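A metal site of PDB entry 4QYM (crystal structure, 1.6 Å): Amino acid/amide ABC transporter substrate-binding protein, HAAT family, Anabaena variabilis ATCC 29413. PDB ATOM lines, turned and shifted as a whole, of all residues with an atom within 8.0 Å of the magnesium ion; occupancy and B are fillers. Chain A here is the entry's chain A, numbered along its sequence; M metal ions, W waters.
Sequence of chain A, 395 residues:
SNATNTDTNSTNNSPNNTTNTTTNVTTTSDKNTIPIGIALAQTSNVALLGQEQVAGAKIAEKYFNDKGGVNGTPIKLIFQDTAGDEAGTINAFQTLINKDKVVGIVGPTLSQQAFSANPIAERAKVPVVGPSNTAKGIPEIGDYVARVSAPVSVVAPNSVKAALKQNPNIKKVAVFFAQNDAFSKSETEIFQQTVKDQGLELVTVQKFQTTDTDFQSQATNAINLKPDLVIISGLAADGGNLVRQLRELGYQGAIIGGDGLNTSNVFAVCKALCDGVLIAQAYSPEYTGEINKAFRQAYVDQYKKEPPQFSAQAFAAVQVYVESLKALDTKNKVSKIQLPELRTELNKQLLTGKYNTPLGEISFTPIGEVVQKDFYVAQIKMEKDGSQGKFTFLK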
ATOM      1  N   GLU A 122      30.267  23.978 -34.741  1.00  0.00           N
ATOM      2  CA  GLU A 122      30.819  23.265 -33.591  1.00  0.00           C
ATOM      3  C   GLU A 122      32.291  22.947 -33.800  1.00  0.00           C
ATOM      4  O   GLU A 122      33.140  23.228 -32.945  1.00  0.00           O
ATOM      5  CB  GLU A 122      30.063  21.970 -33.331  1.00  0.00           C
ATOM      6  CG  GLU A 122      30.667  21.111 -32.224  1.00  0.00           C
ATOM      7  CD  GLU A 122      30.425  21.672 -30.845  1.00  0.00           C
ATOM      8  OE1 GLU A 122      29.584  22.578 -30.726  1.00  0.00           O
ATOM      9  OE2 GLU A 122      31.064  21.193 -29.871  1.00  0.00           O
ATOM     10  N   VAL A 128      26.659  29.078 -31.914  1.00  0.00           N
ATOM     11  CA  VAL A 128      25.399  29.196 -32.623  1.00  0.00           C
ATOM     12  C   VAL A 128      24.311  29.257 -31.567  1.00  0.00           C
ATOM     13  O   VAL A 128      24.285  28.454 -30.632  1.00  0.00           O
ATOM     14  CB  VAL A 128      25.117  27.956 -33.501  1.00  0.00           C
ATOM     15  CG1 VAL A 128      23.711  28.029 -34.105  1.00  0.00           C
ATOM     16  CG2 VAL A 128      26.140  27.838 -34.581  1.00  0.00           C
ATOM     17  N   GLY A 137      17.205  17.103 -29.474  1.00  0.00           N
ATOM     18  CA  GLY A 137      18.595  16.829 -29.780  1.00  0.00           C
ATOM     19  C   GLY A 137      19.438  17.979 -30.287  1.00  0.00           C
ATOM     20  O   GLY A 137      20.634  17.809 -30.536  1.00  0.00           O
ATOM     21  N   ILE A 138      18.848  19.148 -30.474  1.00  0.00           N
ATOM     22  CA  ILE A 138      19.603  20.285 -30.995  1.00  0.00           C
ATOM     23  C   ILE A 138      20.798  20.727 -30.105  1.00  0.00           C
ATOM     24  O   ILE A 138      21.923  20.768 -30.583  1.00  0.00           O
ATOM     25  CB  ILE A 138      18.668  21.477 -31.373  1.00  0.00           C
ATOM     26  CG1 ILE A 138      17.740  21.093 -32.522  1.00  0.00           C
ATOM     27  CG2 ILE A 138      19.489  22.720 -31.702  1.00  0.00           C
ATOM     28  CD1 ILE A 138      18.420  21.069 -33.855  1.00  0.00           C
ATOM     29  N   PRO A 139      20.560  21.053 -28.815  1.00  0.00           N
ATOM     30  CA  PRO A 139      21.683  21.473 -27.960  1.00  0.00           C
ATOM     31  C   PRO A 139      22.757  20.394 -27.839  1.00  0.00           C
ATOM     32  O   PRO A 139      23.943  20.701 -27.649  1.00  0.00           O
ATOM     33  CB  PRO A 139      21.041  21.700 -26.596  1.00  0.00           C
ATOM     34  CG  PRO A 139      19.603  21.832 -26.832  1.00  0.00           C
ATOM     35  CD  PRO A 139      19.283  21.072 -28.077  1.00  0.00           C
ATOM     36  N   GLU A 140      22.334  19.131 -27.946  1.00  0.00           N
ATOM     37  CA  GLU A 140      23.239  17.990 -27.841  1.00  0.00           C
ATOM     38  C   GLU A 140      24.205  17.889 -29.016  1.00  0.00           C
ATOM     39  O   GLU A 140      25.154  17.112 -28.968  1.00  0.00           O
ATOM     40  CB  GLU A 140      22.437  16.700 -27.691  1.00  0.00           C
ATOM     41  CG  GLU A 140      21.760  16.510 -26.326  1.00  0.00           C
ATOM     42  CD  GLU A 140      20.501  17.330 -26.149  1.00  0.00           C
ATOM     43  OE1 GLU A 140      20.014  17.923 -27.139  1.00  0.00           O
ATOM     44  OE2 GLU A 140      19.983  17.384 -25.012  1.00  0.00           O
ATOM     45  N   ILE A 141      23.978  18.678 -30.077  1.00  0.00           N
ATOM     46  CA  ILE A 141      24.888  18.692 -31.218  1.00  0.00           C
ATOM     47  C   ILE A 141      26.325  19.016 -30.795  1.00  0.00           C
ATOM     48  O   ILE A 141      27.282  18.452 -31.314  1.00  0.00           O
ATOM     49  CB  ILE A 141      24.407  19.669 -32.319  1.00  0.00           C
ATOM     50  CG1 ILE A 141      23.115  19.142 -32.961  1.00  0.00           C
ATOM     51  CG2 ILE A 141      25.477  19.844 -33.388  1.00  0.00           C
ATOM     52  CD1 ILE A 141      22.481  20.118 -33.934  1.00  0.00           C
ATOM     53  N   GLY A 142      26.478  19.910 -29.810  1.00  0.00           N
ATOM     54  CA  GLY A 142      27.808  20.194 -29.321  1.00  0.00           C
ATOM     55  C   GLY A 142      27.872  21.322 -28.319  1.00  0.00           C
ATOM     56  O   GLY A 142      26.849  21.911 -27.951  1.00  0.00           O
ATOM     57  N   ASP A 143      29.088  21.627 -27.894  1.00  0.00           N
ATOM     58  CA  ASP A 143      29.333  22.586 -26.821  1.00  0.00           C
ATOM     59  C   ASP A 143      29.206  24.035 -27.268  1.00  0.00           C
ATOM     60  O   ASP A 143      29.197  24.946 -26.437  1.00  0.00           O
ATOM     61  CB  ASP A 143      30.718  22.355 -26.207  1.00  0.00           C
ATOM     62  CG  ASP A 143      30.825  21.026 -25.482  1.00  0.00           C
ATOM     63  OD1 ASP A 143      29.826  20.604 -24.872  1.00  0.00           O
ATOM     64  OD2 ASP A 143      31.915  20.429 -25.512  1.00  0.00           O
ATOM     65  N   TYR A 144      29.081  24.247 -28.577  1.00  0.00           N
ATOM     66  CA  TYR A 144      28.904  25.584 -29.154  1.00  0.00           C
ATOM     67  C   TYR A 144      27.488  25.815 -29.653  1.00  0.00           C
ATOM     68  O   TYR A 144      27.202  26.860 -30.240  1.00  0.00           O
ATOM     69  CB  TYR A 144      29.919  25.822 -30.289  1.00  0.00           C
ATOM     70  CG  TYR A 144      31.291  26.091 -29.753  1.00  0.00           C
ATOM     71  CD1 TYR A 144      32.101  25.051 -29.298  1.00  0.00           C
ATOM     72  CD2 TYR A 144      31.774  27.393 -29.664  1.00  0.00           C
ATOM     73  CE1 TYR A 144      33.361  25.310 -28.776  1.00  0.00           C
ATOM     74  CE2 TYR A 144      33.023  27.660 -29.145  1.00  0.00           C
ATOM     75  CZ  TYR A 144      33.816  26.619 -28.701  1.00  0.00           C
ATOM     76  OH  TYR A 144      35.057  26.890 -28.171  1.00  0.00           O
ATOM     77  N   VAL A 145      26.603  24.845 -29.414  1.00  0.00           N
ATOM     78  CA  VAL A 145      25.214  24.962 -29.856  1.00  0.00           C
ATOM     79  C   VAL A 145      24.246  25.166 -28.687  1.00  0.00           C
ATOM     80  O   VAL A 145      24.103  24.306 -27.825  1.00  0.00           O
ATOM     81  CB  VAL A 145      24.774  23.726 -30.650  1.00  0.00           C
ATOM     82  CG1 VAL A 145      23.339  23.911 -31.135  1.00  0.00           C
ATOM     83  CG2 VAL A 145      25.729  23.481 -31.813  1.00  0.00           C
ATOM     84  N   ALA A 146      23.586  26.321 -28.672  1.00  0.00           N
ATOM     85  CA  ALA A 146      22.545  26.611 -27.701  1.00  0.00           C
ATOM     86  C   ALA A 146      21.293  27.024 -28.464  1.00  0.00           C
ATOM     87  O   ALA A 146      21.345  27.259 -29.680  1.00  0.00           O
ATOM     88  CB  ALA A 146      22.983  27.743 -26.757  1.00  0.00           C
ATOM     89  N   ARG A 147      20.156  27.099 -27.773  1.00  0.00           N
ATOM     90  CA  ARG A 147      18.925  27.600 -28.400  1.00  0.00           C
ATOM     91  C   ARG A 147      18.105  28.323 -27.363  1.00  0.00           C
ATOM     92  O   ARG A 147      18.167  27.982 -26.178  1.00  0.00           O
ATOM     93  CB  ARG A 147      18.101  26.460 -29.025  1.00  0.00           C
ATOM     94  CG  ARG A 147      17.571  25.419 -28.035  1.00  0.00           C
ATOM     95  CD  ARG A 147      16.738  24.371 -28.760  1.00  0.00           C
ATOM     96  NE  ARG A 147      16.503  23.184 -27.947  1.00  0.00           N
ATOM     97  CZ  ARG A 147      16.008  22.044 -28.431  1.00  0.00           C
ATOM     98  NH1 ARG A 147      15.670  21.968 -29.710  1.00  0.00           N
ATOM     99  NH2 ARG A 147      15.841  20.990 -27.639  1.00  0.00           N
ATOM    100  N   ASN A 347      31.096  32.063 -26.269  1.00  0.00           N
ATOM    101  CA  ASN A 347      30.310  30.864 -26.079  1.00  0.00           C
ATOM    102  C   ASN A 347      30.265  30.474 -24.602  1.00  0.00           C
ATOM    103  O   ASN A 347      29.202  30.172 -24.068  1.00  0.00           O
ATOM    104  CB  ASN A 347      30.895  29.708 -26.905  1.00  0.00           C
ATOM    105  CG  ASN A 347      30.065  28.439 -26.802  1.00  0.00           C
ATOM    106  OD1 ASN A 347      28.924  28.397 -27.285  1.00  0.00           O
ATOM    107  ND2 ASN A 347      30.620  27.416 -26.181  1.00  0.00           N
ATOM    108  N   LEU A 351      26.569  30.861 -22.104  1.00  0.00           N
ATOM    109  CA  LEU A 351      25.997  29.713 -21.426  1.00  0.00           C
ATOM    110  C   LEU A 351      25.726  29.965 -19.946  1.00  0.00           C
ATOM    111  O   LEU A 351      24.869  29.308 -19.359  1.00  0.00           O
ATOM    112  CB  LEU A 351      26.877  28.472 -21.604  1.00  0.00           C
ATOM    113  CG  LEU A 351      26.807  27.829 -22.987  1.00  0.00           C
ATOM    114  CD1 LEU A 351      27.939  26.815 -23.125  1.00  0.00           C
ATOM    115  CD2 LEU A 351      25.455  27.172 -23.207  1.00  0.00           C
ATOM    116  N   THR A 365      20.925  25.461 -19.700  1.00  0.00           N
ATOM    117  CA  THR A 365      21.519  24.315 -19.020  1.00  0.00           C
ATOM    118  C   THR A 365      22.973  24.207 -19.464  1.00  0.00           C
ATOM    119  O   THR A 365      23.377  24.876 -20.418  1.00  0.00           O
ATOM    120  CB  THR A 365      20.793  23.011 -19.371  1.00  0.00           C
ATOM    121  OG1 THR A 365      21.179  22.588 -20.689  1.00  0.00           O
ATOM    122  CG2 THR A 365      19.292  23.204 -19.299  1.00  0.00           C
ATOM    123  N   PRO A 366      23.780  23.382 -18.782  1.00  0.00           N
ATOM    124  CA  PRO A 366      25.179  23.272 -19.183  1.00  0.00           C
ATOM    125  C   PRO A 366      25.402  22.852 -20.650  1.00  0.00           C
ATOM    126  O   PRO A 366      26.481  23.096 -21.169  1.00  0.00           O
ATOM    127  CB  PRO A 366      25.722  22.205 -18.232  1.00  0.00           C
ATOM    128  CG  PRO A 366      24.914  22.386 -17.009  1.00  0.00           C
ATOM    129  CD  PRO A 366      23.533  22.731 -17.481  1.00  0.00           C
ATOM    130  N   ILE A 367      24.415  22.241 -21.301  1.00  0.00           N
ATOM    131  CA  ILE A 367      24.571  21.855 -22.711  1.00  0.00           C
ATOM    132  C   ILE A 367      23.847  22.764 -23.706  1.00  0.00           C
ATOM    133  O   ILE A 367      23.745  22.446 -24.882  1.00  0.00           O
ATOM    134  CB  ILE A 367      24.139  20.405 -22.981  1.00  0.00           C
ATOM    135  CG1 ILE A 367      22.687  20.185 -22.562  1.00  0.00           C
ATOM    136  CG2 ILE A 367      25.094  19.456 -22.289  1.00  0.00           C
ATOM    137  CD1 ILE A 367      22.002  19.094 -23.336  1.00  0.00           C
ATOM    138  N   GLY A 368      23.361  23.909 -23.227  1.00  0.00           N
ATOM    139  CA  GLY A 368      22.803  24.913 -24.119  1.00  0.00           C
ATOM    140  C   GLY A 368      21.305  24.782 -24.369  1.00  0.00           C
ATOM    141  O   GLY A 368      20.769  25.429 -25.278  1.00  0.00           O
ATOM    142  N   GLU A 369      20.637  23.959 -23.567  1.00  0.00           N
ATOM    143  CA  GLU A 369      19.183  23.892 -23.625  1.00  0.00           C
ATOM    144  C   GLU A 369      18.597  25.113 -22.908  1.00  0.00           C
ATOM    145  O   GLU A 369      19.146  25.584 -21.907  1.00  0.00           O
ATOM    146  CB  GLU A 369      18.673  22.621 -22.954  1.00  0.00           C
ATOM    147  CG  GLU A 369      17.164  22.443 -23.064  1.00  0.00           C
ATOM    148  CD  GLU A 369      16.705  22.354 -24.500  1.00  0.00           C
ATOM    149  OE1 GLU A 369      16.614  21.224 -25.033  1.00  0.00           O
ATOM    150  OE2 GLU A 369      16.459  23.405 -25.126  1.00  0.00           O
HETATM  151 MG    MG M   1      25.059  22.551 -26.684  1.00  0.00          MG
HETATM  152  O   HOH W   1      26.157  24.194 -25.521  1.00  0.00           O
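The backbone NH (N) of Ile 367 sits close to the side-chain hydroxyl (OG1) of Thr 365.
Four residues have an atom within 4 Å of the magnesium ion: Pro 139, Gly 142, Val 145 and Ile 367.
The nearest printed residue that does not touch the magnesium ion is Gly 368 (4.1 Å).
O of Ile 367 binds the magnesium ion, 2.2 Å away.
The backbone carbonyl oxygen (O) of Gly 142 is bound to the magnesium ion (2.3 Å).
Water W1 binds the magnesium ion (2.3 Å).
The magnesium ion is bound by O of Val 145 (2.3 Å).
O of Pro 139 binds the magnesium ion, 2.4 Å away.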
